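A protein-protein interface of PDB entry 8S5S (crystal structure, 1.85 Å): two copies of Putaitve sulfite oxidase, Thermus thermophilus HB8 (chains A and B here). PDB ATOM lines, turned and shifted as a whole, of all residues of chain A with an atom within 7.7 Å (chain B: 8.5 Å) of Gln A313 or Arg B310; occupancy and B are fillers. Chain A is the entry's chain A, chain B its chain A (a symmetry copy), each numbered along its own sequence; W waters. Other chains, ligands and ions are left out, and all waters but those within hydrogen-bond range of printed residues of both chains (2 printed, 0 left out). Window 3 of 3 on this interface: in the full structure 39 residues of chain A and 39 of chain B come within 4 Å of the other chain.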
ATOM      1  N   VAL A 285      42.419  -4.905 -14.466  1.00  0.00           N
ATOM      2  CA  VAL A 285      42.435  -4.316 -15.793  1.00  0.00           C
ATOM      3  C   VAL A 285      41.621  -3.041 -15.672  1.00  0.00           C
ATOM      4  O   VAL A 285      40.450  -3.109 -15.311  1.00  0.00           O
ATOM      5  CB  VAL A 285      41.897  -5.231 -16.907  1.00  0.00           C
ATOM      6  CG1 VAL A 285      41.899  -4.508 -18.240  1.00  0.00           C
ATOM      7  CG2 VAL A 285      42.706  -6.519 -17.034  1.00  0.00           C
ATOM      8  N   SER A 301      25.056   6.861 -15.160  1.00  0.00           N
ATOM      9  CA  SER A 301      26.101   5.877 -15.043  1.00  0.00           C
ATOM     10  C   SER A 301      26.735   5.590 -16.398  1.00  0.00           C
ATOM     11  O   SER A 301      26.125   5.752 -17.452  1.00  0.00           O
ATOM     12  CB  SER A 301      25.638   4.614 -14.392  1.00  0.00           C
ATOM     13  OG  SER A 301      24.901   3.815 -15.316  1.00  0.00           O
ATOM     14  N   VAL A 302      27.963   5.113 -16.319  1.00  0.00           N
ATOM     15  CA  VAL A 302      28.524   4.310 -17.383  1.00  0.00           C
ATOM     16  C   VAL A 302      28.825   2.962 -16.765  1.00  0.00           C
ATOM     17  O   VAL A 302      29.251   2.909 -15.606  1.00  0.00           O
ATOM     18  CB  VAL A 302      29.792   4.940 -17.954  1.00  0.00           C
ATOM     19  CG1 VAL A 302      30.465   4.025 -18.947  1.00  0.00           C
ATOM     20  CG2 VAL A 302      29.503   6.303 -18.568  1.00  0.00           C
ATOM     21  N   GLU A 303      28.470   1.889 -17.494  1.00  0.00           N
ATOM     22  CA  GLU A 303      28.591   0.549 -16.946  1.00  0.00           C
ATOM     23  C   GLU A 303      29.377  -0.293 -17.910  1.00  0.00           C
ATOM     24  O   GLU A 303      29.322  -0.083 -19.120  1.00  0.00           O
ATOM     25  CB  GLU A 303      27.249  -0.084 -16.593  1.00  0.00           C
ATOM     26  CG  GLU A 303      26.478   0.782 -15.597  1.00  0.00           C
ATOM     27  CD  GLU A 303      25.017   0.405 -15.433  1.00  0.00           C
ATOM     28  OE1 GLU A 303      24.647  -0.709 -15.864  1.00  0.00           O
ATOM     29  OE2 GLU A 303      24.265   1.208 -14.840  1.00  0.00           O
ATOM     30  N   VAL A 304      30.158  -1.231 -17.375  1.00  0.00           N
ATOM     31  CA  VAL A 304      30.923  -2.101 -18.243  1.00  0.00           C
ATOM     32  C   VAL A 304      30.604  -3.563 -17.938  1.00  0.00           C
ATOM     33  O   VAL A 304      30.237  -3.949 -16.829  1.00  0.00           O
ATOM     34  CB  VAL A 304      32.419  -1.828 -18.094  1.00  0.00           C
ATOM     35  CG1 VAL A 304      32.734  -0.358 -18.333  1.00  0.00           C
ATOM     36  CG2 VAL A 304      32.904  -2.248 -16.741  1.00  0.00           C
ATOM     37  N   SER A 305      30.737  -4.400 -18.956  1.00  0.00           N
ATOM     38  CA  SER A 305      30.519  -5.820 -18.750  1.00  0.00           C
ATOM     39  C   SER A 305      31.625  -6.558 -19.472  1.00  0.00           C
ATOM     40  O   SER A 305      31.977  -6.174 -20.584  1.00  0.00           O
ATOM     41  CB  SER A 305      29.158  -6.284 -19.244  1.00  0.00           C
ATOM     42  OG  SER A 305      29.014  -7.695 -19.134  1.00  0.00           O
ATOM     43  N   ALA A 306      32.160  -7.599 -18.817  1.00  0.00           N
ATOM     44  CA  ALA A 306      33.124  -8.461 -19.482  1.00  0.00           C
ATOM     45  C   ALA A 306      32.568  -9.867 -19.713  1.00  0.00           C
ATOM     46  O   ALA A 306      33.327 -10.756 -20.101  1.00  0.00           O
ATOM     47  CB  ALA A 306      34.410  -8.506 -18.692  1.00  0.00           C
ATOM     48  N   ASN A 307      31.254 -10.052 -19.496  1.00  0.00           N
ATOM     49  CA  ASN A 307      30.617 -11.364 -19.606  1.00  0.00           C
ATOM     50  C   ASN A 307      29.387 -11.279 -20.477  1.00  0.00           C
ATOM     51  O   ASN A 307      28.446 -12.025 -20.279  1.00  0.00           O
ATOM     52  CB  ASN A 307      30.320 -11.972 -18.252  1.00  0.00           C
ATOM     53  CG  ASN A 307      29.460 -11.083 -17.403  1.00  0.00           C
ATOM     54  OD1 ASN A 307      28.724 -10.239 -17.931  1.00  0.00           O
ATOM     55  ND2 ASN A 307      29.428 -11.360 -16.122  1.00  0.00           N
ATOM     56  N   THR A 311      26.446  -9.515 -16.244  1.00  0.00           N
ATOM     57  CA  THR A 311      26.561  -8.599 -15.127  1.00  0.00           C
ATOM     58  C   THR A 311      27.189  -7.333 -15.663  1.00  0.00           C
ATOM     59  O   THR A 311      27.982  -7.363 -16.606  1.00  0.00           O
ATOM     60  CB  THR A 311      27.371  -9.129 -13.939  1.00  0.00           C
ATOM     61  OG1 THR A 311      28.646  -9.392 -14.511  1.00  0.00           O
ATOM     62  CG2 THR A 311      26.789 -10.405 -13.364  1.00  0.00           C
ATOM     63  N   TRP A 312      26.758  -6.221 -15.069  1.00  0.00           N
ATOM     64  CA  TRP A 312      27.269  -4.910 -15.428  1.00  0.00           C
ATOM     65  C   TRP A 312      27.805  -4.265 -14.155  1.00  0.00           C
ATOM     66  O   TRP A 312      27.149  -4.338 -13.099  1.00  0.00           O
ATOM     67  CB  TRP A 312      26.177  -4.028 -16.051  1.00  0.00           C
ATOM     68  CG  TRP A 312      25.755  -4.391 -17.448  1.00  0.00           C
ATOM     69  CD1 TRP A 312      24.716  -5.225 -17.724  1.00  0.00           C
ATOM     70  CD2 TRP A 312      26.285  -3.950 -18.727  1.00  0.00           C
ATOM     71  NE1 TRP A 312      24.593  -5.369 -19.075  1.00  0.00           N
ATOM     72  CE2 TRP A 312      25.528  -4.609 -19.715  1.00  0.00           C
ATOM     73  CE3 TRP A 312      27.316  -3.090 -19.147  1.00  0.00           C
ATOM     74  CZ2 TRP A 312      25.739  -4.420 -21.072  1.00  0.00           C
ATOM     75  CZ3 TRP A 312      27.519  -2.895 -20.490  1.00  0.00           C
ATOM     76  CH2 TRP A 312      26.773  -3.580 -21.439  1.00  0.00           C
ATOM     77  N   GLN A 313      28.980  -3.638 -14.275  1.00  0.00           N
ATOM     78  CA  GLN A 313      29.625  -2.952 -13.159  1.00  0.00           C
ATOM     79  C   GLN A 313      29.697  -1.445 -13.425  1.00  0.00           C
ATOM     80  O   GLN A 313      30.118  -1.022 -14.505  1.00  0.00           O
ATOM     81  CB  GLN A 313      31.012  -3.544 -12.962  1.00  0.00           C
ATOM     82  CG  GLN A 313      31.758  -2.979 -11.762  1.00  0.00           C
ATOM     83  CD  GLN A 313      33.179  -3.500 -11.697  1.00  0.00           C
ATOM     84  OE1 GLN A 313      33.423  -4.692 -11.892  1.00  0.00           O
ATOM     85  NE2 GLN A 313      34.143  -2.607 -11.524  1.00  0.00           N
ATOM     86  N   GLN A 314      29.259  -0.656 -12.435  1.00  0.00           N
ATOM     87  CA  GLN A 314      29.270   0.796 -12.551  1.00  0.00           C
ATOM     88  C   GLN A 314      30.717   1.297 -12.643  1.00  0.00           C
ATOM     89  O   GLN A 314      31.566   0.927 -11.831  1.00  0.00           O
ATOM     90  CB  GLN A 314      28.524   1.369 -11.357  1.00  0.00           C
ATOM     91  CG  GLN A 314      28.247   2.859 -11.500  1.00  0.00           C
ATOM     92  CD  GLN A 314      27.347   3.432 -10.429  1.00  0.00           C
ATOM     93  OE1 GLN A 314      26.577   4.363 -10.667  1.00  0.00           O
ATOM     94  NE2 GLN A 314      27.507   2.957  -9.216  1.00  0.00           N
ATOM     95  N   ALA A 315      31.021   2.121 -13.649  1.00  0.00           N
ATOM     96  CA  ALA A 315      32.283   2.841 -13.708  1.00  0.00           C
ATOM     97  C   ALA A 315      32.203   4.048 -12.813  1.00  0.00           C
ATOM     98  O   ALA A 315      31.113   4.460 -12.440  1.00  0.00           O
ATOM     99  CB  ALA A 315      32.608   3.278 -15.106  1.00  0.00           C
ATOM    100  N   ARG A 316      33.376   4.605 -12.515  1.00  0.00           N
ATOM    101  CA  ARG A 316      33.516   5.893 -11.859  1.00  0.00           C
ATOM    102  C   ARG A 316      33.675   7.012 -12.892  1.00  0.00           C
ATOM    103  O   ARG A 316      34.554   6.984 -13.736  1.00  0.00           O
ATOM    104  CB  ARG A 316      34.802   5.970 -11.036  1.00  0.00           C
ATOM    105  CG  ARG A 316      34.591   5.609  -9.583  1.00  0.00           C
ATOM    106  CD  ARG A 316      33.940   6.735  -8.756  1.00  0.00           C
ATOM    107  NE  ARG A 316      33.487   6.067  -7.527  1.00  0.00           N
ATOM    108  CZ  ARG A 316      34.264   5.276  -6.784  1.00  0.00           C
ATOM    109  NH1 ARG A 316      33.731   4.270  -6.108  1.00  0.00           N
ATOM    110  NH2 ARG A 316      35.582   5.391  -6.845  1.00  0.00           N
ATOM    111  N   TRP A 329      35.620   8.304 -17.681  1.00  0.00           N
ATOM    112  CA  TRP A 329      35.219   7.246 -16.769  1.00  0.00           C
ATOM    113  C   TRP A 329      36.295   6.161 -16.724  1.00  0.00           C
ATOM    114  O   TRP A 329      37.038   5.960 -17.684  1.00  0.00           O
ATOM    115  CB  TRP A 329      33.854   6.644 -17.161  1.00  0.00           C
ATOM    116  CG  TRP A 329      33.773   6.028 -18.537  1.00  0.00           C
ATOM    117  CD1 TRP A 329      33.294   6.668 -19.644  1.00  0.00           C
ATOM    118  CD2 TRP A 329      34.128   4.704 -18.975  1.00  0.00           C
ATOM    119  NE1 TRP A 329      33.360   5.858 -20.732  1.00  0.00           N
ATOM    120  CE2 TRP A 329      33.870   4.651 -20.359  1.00  0.00           C
ATOM    121  CE3 TRP A 329      34.673   3.570 -18.354  1.00  0.00           C
ATOM    122  CZ2 TRP A 329      34.119   3.516 -21.117  1.00  0.00           C
ATOM    123  CZ3 TRP A 329      34.922   2.445 -19.100  1.00  0.00           C
ATOM    124  CH2 TRP A 329      34.647   2.419 -20.465  1.00  0.00           C
ATOM    125  N   GLN A 330      36.272   5.407 -15.623  1.00  0.00           N
ATOM    126  CA  GLN A 330      37.105   4.213 -15.529  1.00  0.00           C
ATOM    127  C   GLN A 330      36.362   3.160 -14.710  1.00  0.00           C
ATOM    128  O   GLN A 330      35.670   3.481 -13.755  1.00  0.00           O
ATOM    129  CB  GLN A 330      38.462   4.490 -14.875  1.00  0.00           C
ATOM    130  CG  GLN A 330      38.373   4.828 -13.391  1.00  0.00           C
ATOM    131  CD  GLN A 330      38.412   3.630 -12.448  1.00  0.00           C
ATOM    132  OE1 GLN A 330      38.571   2.474 -12.835  1.00  0.00           O
ATOM    133  NE2 GLN A 330      38.256   3.900 -11.165  1.00  0.00           N
ATOM    134  N   ALA A 331      36.576   1.911 -15.095  1.00  0.00           N
ATOM    135  CA  ALA A 331      36.140   0.785 -14.297  1.00  0.00           C
ATOM    136  C   ALA A 331      37.280  -0.227 -14.252  1.00  0.00           C
ATOM    137  O   ALA A 331      37.803  -0.623 -15.289  1.00  0.00           O
ATOM    138  CB  ALA A 331      34.889   0.161 -14.874  1.00  0.00           C
ATOM    139  N   THR A 332      37.596  -0.678 -13.028  1.00  0.00           N
ATOM    140  CA  THR A 332      38.711  -1.589 -12.848  1.00  0.00           C
ATOM    141  C   THR A 332      38.129  -2.975 -12.586  1.00  0.00           C
ATOM    142  O   THR A 332      37.343  -3.139 -11.671  1.00  0.00           O
ATOM    143  CB  THR A 332      39.602  -1.089 -11.706  1.00  0.00           C
ATOM    144  OG1 THR A 332      40.124   0.156 -12.175  1.00  0.00           O
ATOM    145  CG2 THR A 332      40.776  -2.012 -11.447  1.00  0.00           C
ATOM    146  N   LEU A 333      38.521  -3.920 -13.411  1.00  0.00           N
ATOM    147  CA  LEU A 333      37.979  -5.270 -13.404  1.00  0.00           C
ATOM    148  C   LEU A 333      39.082  -6.259 -13.054  1.00  0.00           C
ATOM    149  O   LEU A 333      40.211  -6.126 -13.556  1.00  0.00           O
ATOM    150  CB  LEU A 333      37.494  -5.615 -14.803  1.00  0.00           C
ATOM    151  CG  LEU A 333      36.446  -4.699 -15.434  1.00  0.00           C
ATOM    152  CD1 LEU A 333      36.209  -5.254 -16.836  1.00  0.00           C
ATOM    153  CD2 LEU A 333      35.200  -4.664 -14.606  1.00  0.00           C
ATOM    154  N   TYR A 334      38.685  -7.304 -12.318  1.00  0.00           N
ATOM    155  CA  TYR A 334      39.520  -8.471 -12.054  1.00  0.00           C
ATOM    156  C   TYR A 334      39.295  -9.503 -13.159  1.00  0.00           C
ATOM    157  O   TYR A 334      38.189 -10.011 -13.286  1.00  0.00           O
ATOM    158  CB  TYR A 334      39.097  -9.001 -10.680  1.00  0.00           C
ATOM    159  CG  TYR A 334      39.921 -10.210 -10.265  1.00  0.00           C
ATOM    160  CD1 TYR A 334      41.141 -10.039  -9.617  1.00  0.00           C
ATOM    161  CD2 TYR A 334      39.512 -11.510 -10.559  1.00  0.00           C
ATOM    162  CE1 TYR A 334      41.921 -11.123  -9.251  1.00  0.00           C
ATOM    163  CE2 TYR A 334      40.285 -12.604 -10.200  1.00  0.00           C
ATOM    164  CZ  TYR A 334      41.491 -12.404  -9.544  1.00  0.00           C
ATOM    165  OH  TYR A 334      42.284 -13.439  -9.172  1.00  0.00           O
ATOM    166  N   MET A 343      32.496  -4.412 -22.857  1.00  0.00           N
ATOM    167  CA  MET A 343      31.566  -3.500 -23.487  1.00  0.00           C
ATOM    168  C   MET A 343      31.200  -2.402 -22.500  1.00  0.00           C
ATOM    169  O   MET A 343      31.232  -2.613 -21.290  1.00  0.00           O
ATOM    170  CB  MET A 343      30.385  -4.282 -24.080  1.00  0.00           C
ATOM    171  CG  MET A 343      29.563  -5.137 -23.182  1.00  0.00           C
ATOM    172  SD  MET A 343      28.300  -6.094 -24.092  1.00  0.00           S
ATOM    173  CE  MET A 343      29.491  -7.361 -24.534  1.00  0.00           C
ATOM    174  N   ARG A 345      28.357   0.939 -21.677  1.00  0.00           N
ATOM    175  CA  ARG A 345      27.008   1.426 -21.893  1.00  0.00           C
ATOM    176  C   ARG A 345      26.791   2.653 -21.028  1.00  0.00           C
ATOM    177  O   ARG A 345      27.006   2.598 -19.825  1.00  0.00           O
ATOM    178  CB  ARG A 345      26.021   0.333 -21.466  1.00  0.00           C
ATOM    179  CG  ARG A 345      24.546   0.617 -21.641  1.00  0.00           C
ATOM    180  CD  ARG A 345      23.629  -0.545 -21.117  1.00  0.00           C
ATOM    181  NE  ARG A 345      23.831  -0.857 -19.700  1.00  0.00           N
ATOM    182  CZ  ARG A 345      23.296  -1.929 -19.143  1.00  0.00           C
ATOM    183  NH1 ARG A 345      22.563  -2.762 -19.862  1.00  0.00           N
ATOM    184  NH2 ARG A 345      23.456  -2.178 -17.874  1.00  0.00           N
ATOM    185  N   GLU B 303      17.242  -6.034 -15.673  1.00  0.00           N
ATOM    186  CA  GLU B 303      18.397  -6.177 -14.803  1.00  0.00           C
ATOM    187  C   GLU B 303      17.997  -5.783 -13.409  1.00  0.00           C
ATOM    188  O   GLU B 303      17.135  -4.928 -13.219  1.00  0.00           O
ATOM    189  CB  GLU B 303      19.619  -5.405 -15.289  1.00  0.00           C
ATOM    190  CG  GLU B 303      20.017  -5.837 -16.700  1.00  0.00           C
ATOM    191  CD  GLU B 303      21.008  -4.915 -17.385  1.00  0.00           C
ATOM    192  OE1 GLU B 303      21.626  -4.088 -16.678  1.00  0.00           O
ATOM    193  OE2 GLU B 303      21.188  -5.054 -18.615  1.00  0.00           O
ATOM    194  N   VAL B 304      18.592  -6.443 -12.415  1.00  0.00           N
ATOM    195  CA  VAL B 304      18.279  -6.099 -11.045  1.00  0.00           C
ATOM    196  C   VAL B 304      19.557  -5.750 -10.284  1.00  0.00           C
ATOM    197  O   VAL B 304      20.657  -6.215 -10.577  1.00  0.00           O
ATOM    198  CB  VAL B 304      17.533  -7.243 -10.360  1.00  0.00           C
ATOM    199  CG1 VAL B 304      16.293  -7.638 -11.148  1.00  0.00           C
ATOM    200  CG2 VAL B 304      18.430  -8.428 -10.176  1.00  0.00           C
ATOM    201  N   SER B 305      19.409  -4.896  -9.282  1.00  0.00           N
ATOM    202  CA  SER B 305      20.554  -4.552  -8.459  1.00  0.00           C
ATOM    203  C   SER B 305      20.095  -4.567  -7.016  1.00  0.00           C
ATOM    204  O   SER B 305      19.001  -4.088  -6.729  1.00  0.00           O
ATOM    205  CB  SER B 305      21.150  -3.198  -8.815  1.00  0.00           C
ATOM    206  OG  SER B 305      22.196  -2.836  -7.922  1.00  0.00           O
ATOM    207  N   ALA B 306      20.939  -5.127  -6.139  1.00  0.00           N
ATOM    208  CA  ALA B 306      20.659  -5.060  -4.713  1.00  0.00           C
ATOM    209  C   ALA B 306      21.673  -4.185  -3.974  1.00  0.00           C
ATOM    210  O   ALA B 306      21.674  -4.177  -2.742  1.00  0.00           O
ATOM    211  CB  ALA B 306      20.611  -6.451  -4.129  1.00  0.00           C
ATOM    212  N   ASN B 307      22.508  -3.444  -4.723  1.00  0.00           N
ATOM    213  CA  ASN B 307      23.572  -2.628  -4.138  1.00  0.00           C
ATOM    214  C   ASN B 307      23.520  -1.225  -4.692  1.00  0.00           C
ATOM    215  O   ASN B 307      24.543  -0.572  -4.800  1.00  0.00           O
ATOM    216  CB  ASN B 307      24.937  -3.261  -4.305  1.00  0.00           C
ATOM    217  CG  ASN B 307      25.267  -3.535  -5.743  1.00  0.00           C
ATOM    218  OD1 ASN B 307      24.718  -2.885  -6.643  1.00  0.00           O
ATOM    219  ND2 ASN B 307      26.256  -4.368  -5.961  1.00  0.00           N
ATOM    220  N   GLY B 308      22.301  -0.778  -4.983  1.00  0.00           N
ATOM    221  CA  GLY B 308      22.032   0.596  -5.321  1.00  0.00           C
ATOM    222  C   GLY B 308      22.566   0.951  -6.695  1.00  0.00           C
ATOM    223  O   GLY B 308      22.753   2.124  -6.962  1.00  0.00           O
ATOM    224  N   GLY B 309      22.815  -0.036  -7.559  1.00  0.00           N
ATOM    225  CA  GLY B 309      23.268   0.233  -8.912  1.00  0.00           C
ATOM    226  C   GLY B 309      24.774   0.085  -9.119  1.00  0.00           C
ATOM    227  O   GLY B 309      25.296   0.280 -10.234  1.00  0.00           O
ATOM    228  N   ARG B 310      25.485  -0.380  -8.100  1.00  0.00           N
ATOM    229  CA  ARG B 310      26.911  -0.583  -8.284  1.00  0.00           C
ATOM    230  C   ARG B 310      27.156  -1.762  -9.213  1.00  0.00           C
ATOM    231  O   ARG B 310      28.126  -1.738  -9.988  1.00  0.00           O
ATOM    232  CB  ARG B 310      27.672  -0.730  -6.958  1.00  0.00           C
ATOM    233  CG  ARG B 310      27.588   0.549  -6.121  1.00  0.00           C
ATOM    234  CD  ARG B 310      28.446   0.597  -4.806  1.00  0.00           C
ATOM    235  NE  ARG B 310      28.281  -0.547  -3.890  1.00  0.00           N
ATOM    236  CZ  ARG B 310      28.785  -1.793  -4.057  1.00  0.00           C
ATOM    237  NH1 ARG B 310      29.643  -2.069  -5.038  1.00  0.00           N
ATOM    238  NH2 ARG B 310      28.426  -2.767  -3.225  1.00  0.00           N
ATOM    239  N   THR B 311      26.302  -2.803  -9.102  1.00  0.00           N
ATOM    240  CA  THR B 311      26.351  -3.910 -10.037  1.00  0.00           C
ATOM    241  C   THR B 311      24.920  -4.243 -10.394  1.00  0.00           C
ATOM    242  O   THR B 311      24.004  -4.070  -9.586  1.00  0.00           O
ATOM    243  CB  THR B 311      27.073  -5.159  -9.523  1.00  0.00           C
ATOM    244  OG1 THR B 311      26.325  -5.508  -8.365  1.00  0.00           O
ATOM    245  CG2 THR B 311      28.513  -4.880  -9.142  1.00  0.00           C
ATOM    246  N   TRP B 312      24.759  -4.666 -11.646  1.00  0.00           N
ATOM    247  CA  TRP B 312      23.460  -5.063 -12.161  1.00  0.00           C
ATOM    248  C   TRP B 312      23.595  -6.487 -12.689  1.00  0.00           C
ATOM    249  O   TRP B 312      24.587  -6.805 -13.372  1.00  0.00           O
ATOM    250  CB  TRP B 312      22.984  -4.125 -13.281  1.00  0.00           C
ATOM    251  CG  TRP B 312      22.541  -2.756 -12.846  1.00  0.00           C
ATOM    252  CD1 TRP B 312      23.369  -1.677 -12.805  1.00  0.00           C
ATOM    253  CD2 TRP B 312      21.228  -2.287 -12.438  1.00  0.00           C
ATOM    254  NE1 TRP B 312      22.679  -0.589 -12.357  1.00  0.00           N
ATOM    255  CE2 TRP B 312      21.376  -0.921 -12.126  1.00  0.00           C
ATOM    256  CE3 TRP B 312      19.953  -2.865 -12.288  1.00  0.00           C
ATOM    257  CZ2 TRP B 312      20.319  -0.128 -11.710  1.00  0.00           C
ATOM    258  CZ3 TRP B 312      18.906  -2.078 -11.885  1.00  0.00           C
ATOM    259  CH2 TRP B 312      19.090  -0.740 -11.560  1.00  0.00           C
ATOM    260  N   GLN B 313      22.595  -7.316 -12.375  1.00  0.00           N
ATOM    261  CA  GLN B 313      22.557  -8.709 -12.817  1.00  0.00           C
ATOM    262  C   GLN B 313      21.384  -8.936 -13.774  1.00  0.00           C
ATOM    263  O   GLN B 313      20.255  -8.536 -13.482  1.00  0.00           O
ATOM    264  CB  GLN B 313      22.450  -9.603 -11.591  1.00  0.00           C
ATOM    265  CG  GLN B 313      22.498 -11.090 -11.907  1.00  0.00           C
ATOM    266  CD  GLN B 313      22.248 -11.930 -10.671  1.00  0.00           C
ATOM    267  OE1 GLN B 313      22.792 -11.651  -9.601  1.00  0.00           O
ATOM    268  NE2 GLN B 313      21.351 -12.900 -10.770  1.00  0.00           N
ATOM    269  N   MET B 343      16.220  -3.223  -6.970  1.00  0.00           N
ATOM    270  CA  MET B 343      15.650  -2.392  -8.008  1.00  0.00           C
ATOM    271  C   MET B 343      15.711  -3.137  -9.333  1.00  0.00           C
ATOM    272  O   MET B 343      16.584  -3.977  -9.537  1.00  0.00           O
ATOM    273  CB  MET B 343      16.311  -1.006  -7.993  1.00  0.00           C
ATOM    274  CG  MET B 343      17.785  -0.908  -8.167  1.00  0.00           C
ATOM    275  SD  MET B 343      18.399   0.802  -7.977  1.00  0.00           S
ATOM    276  CE  MET B 343      18.419   0.662  -6.189  1.00  0.00           C
ATOM    277  N   ARG B 345      15.314  -2.713 -13.758  1.00  0.00           N
ATOM    278  CA  ARG B 345      15.460  -1.804 -14.879  1.00  0.00           C
ATOM    279  C   ARG B 345      15.297  -2.590 -16.166  1.00  0.00           C
ATOM    280  O   ARG B 345      15.984  -3.582 -16.366  1.00  0.00           O
ATOM    281  CB  ARG B 345      16.869  -1.202 -14.837  1.00  0.00           C
ATOM    282  CG  ARG B 345      17.230  -0.190 -15.901  1.00  0.00           C
ATOM    283  CD  ARG B 345      18.713   0.314 -15.796  1.00  0.00           C
ATOM    284  NE  ARG B 345      19.704  -0.761 -15.886  1.00  0.00           N
ATOM    285  CZ  ARG B 345      20.981  -0.549 -15.618  1.00  0.00           C
ATOM    286  NH1 ARG B 345      21.399   0.649 -15.250  1.00  0.00           N
ATOM    287  NH2 ARG B 345      21.859  -1.506 -15.734  1.00  0.00           N
HETATM  288  O   HOH W   1      24.299   2.020 -12.246  1.00  0.00           O
HETATM  289  O   HOH W   2      22.256  -7.143 -19.984  1.00  0.00           O
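The indole nitrogen (NE1) of Trp B312 sits at hydrogen-bond distance from the side-chain carboxylate (OE2) of Glu A303, 3.5 Å away.
The guanidinium group (NH2) of Arg B345 is in salt-bridge range of the side-chain carboxylate (OE1) of Glu A303, at 2.9 Å.
NE1 of Trp A312 is in hydrogen-bond range of OE2 of Glu B303 (3.5 Å).
O of Trp A312 is in hydrogen-bond range of N of Trp B312 (2.8 Å).
O of Arg B310 lies within hydrogen-bond range of N of Gln A314 (2.9 Å).
The guanidinium group (NH2) of Arg A345 is in salt-bridge range of the side-chain carboxylate (OE1) of Glu B303, 2.9 Å away.
The guanidinium group (NH2) of Arg A345 lies close to the guanidinium group (NH2) of Arg B345 (2.8 Å).
OE1 of Glu A303 is in salt-bridge range of NH2 of Arg A345 (2.8 Å).
NE2 of Gln A313 sits at hydrogen-bond distance from O of Thr A332, at 3.2 Å.
The side-chain carboxylate (OE1) of Glu B303 is in salt-bridge range of the guanidinium group (NH2) of Arg B345, 2.8 Å away.
The backbone NH (N) of Gly B309 sits at hydrogen-bond distance from the side-chain hydroxyl (OG) of Ser B305 (2.9 Å).
The side-chain hydroxyl (OG1) of Thr B311 sits at hydrogen-bond distance from the side-chain amide nitrogen (ND2) of Asn B307 (2.7 Å).
The indole nitrogen of Trp B312 is in hydrogen-bond range of the backbone carbonyl oxygen of Gly B309 (3.5 Å).
Thr A311 touches Trp B312.
Trp A312 touches Thr B311 (O to CA, 3.2 Å).
Arg B310 touches Gln A313.
CB of Gln A314 touches O of Gly B309, 3.6 Å away.
Gln A313 touches just one residue of chain B: Arg B310 (3.7 Å).
Arg B310 touches just these residues of chain A: Gln A313 (3.7 Å) and Gln A314 (2.9 Å).
Gly B309 touches just one residue of chain A: Gln A314 (3.6 Å).
Printed residues of chain B within 4 Å of Trp A312: Glu B303, Thr B311 and Trp B312.
Printed residues of chain A within 4 Å of Arg B345: Glu A303 (2.9 Å) and Arg A345 (2.8 Å).
Ala A331 touches none of the printed residues of chain B.
The nearest residue of chain B that does not touch Gln A313 is Thr B311 (4.6 Å).
The nearest residue of chain A that does not touch Arg B310 is Trp A312 (4.2 Å).
The nearest printed residue of chain A that does not touch Arg B345 is Ser A301 (4.7 Å).
Of the 22 printed residues of chain A, 6 touch a printed residue of chain B.
Hydrophobic or aromatic side chains of chain A within 4 Å of the printed part of chain B: Trp A312.
Of the 13 printed residues of chain B, 6 touch a printed residue of chain A.
Along chain B the printed residues that touch a printed residue of chain A span positions 303 to 345.
Glu A303 touches Trp B312, and with the chains exchanged Trp A312 touches Glu B303.
Thr A311 touches Trp B312, and with the chains exchanged Trp A312 touches Thr B311.
Trp A312 touches its own counterpart, Trp B312.
Arg B345 touches its own counterpart, Arg A345.
Of the 11 pairs that touch across the chains among the printed residues, 8 have their exchanged pair printed and touching as well.
Water W2 lies within hydrogen-bond range of OE2 of Glu B303 (2.7 Å) and NE1 of Trp A312 (3.1 Å).
Water W1 lies within hydrogen-bond range of the side-chain carboxylate (OE2) of Glu A303 (2.7 Å), the backbone carbonyl oxygen (O) of Gly B309 (2.8 Å) and the indole nitrogen (NE1) of Trp B312 (3.1 Å).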
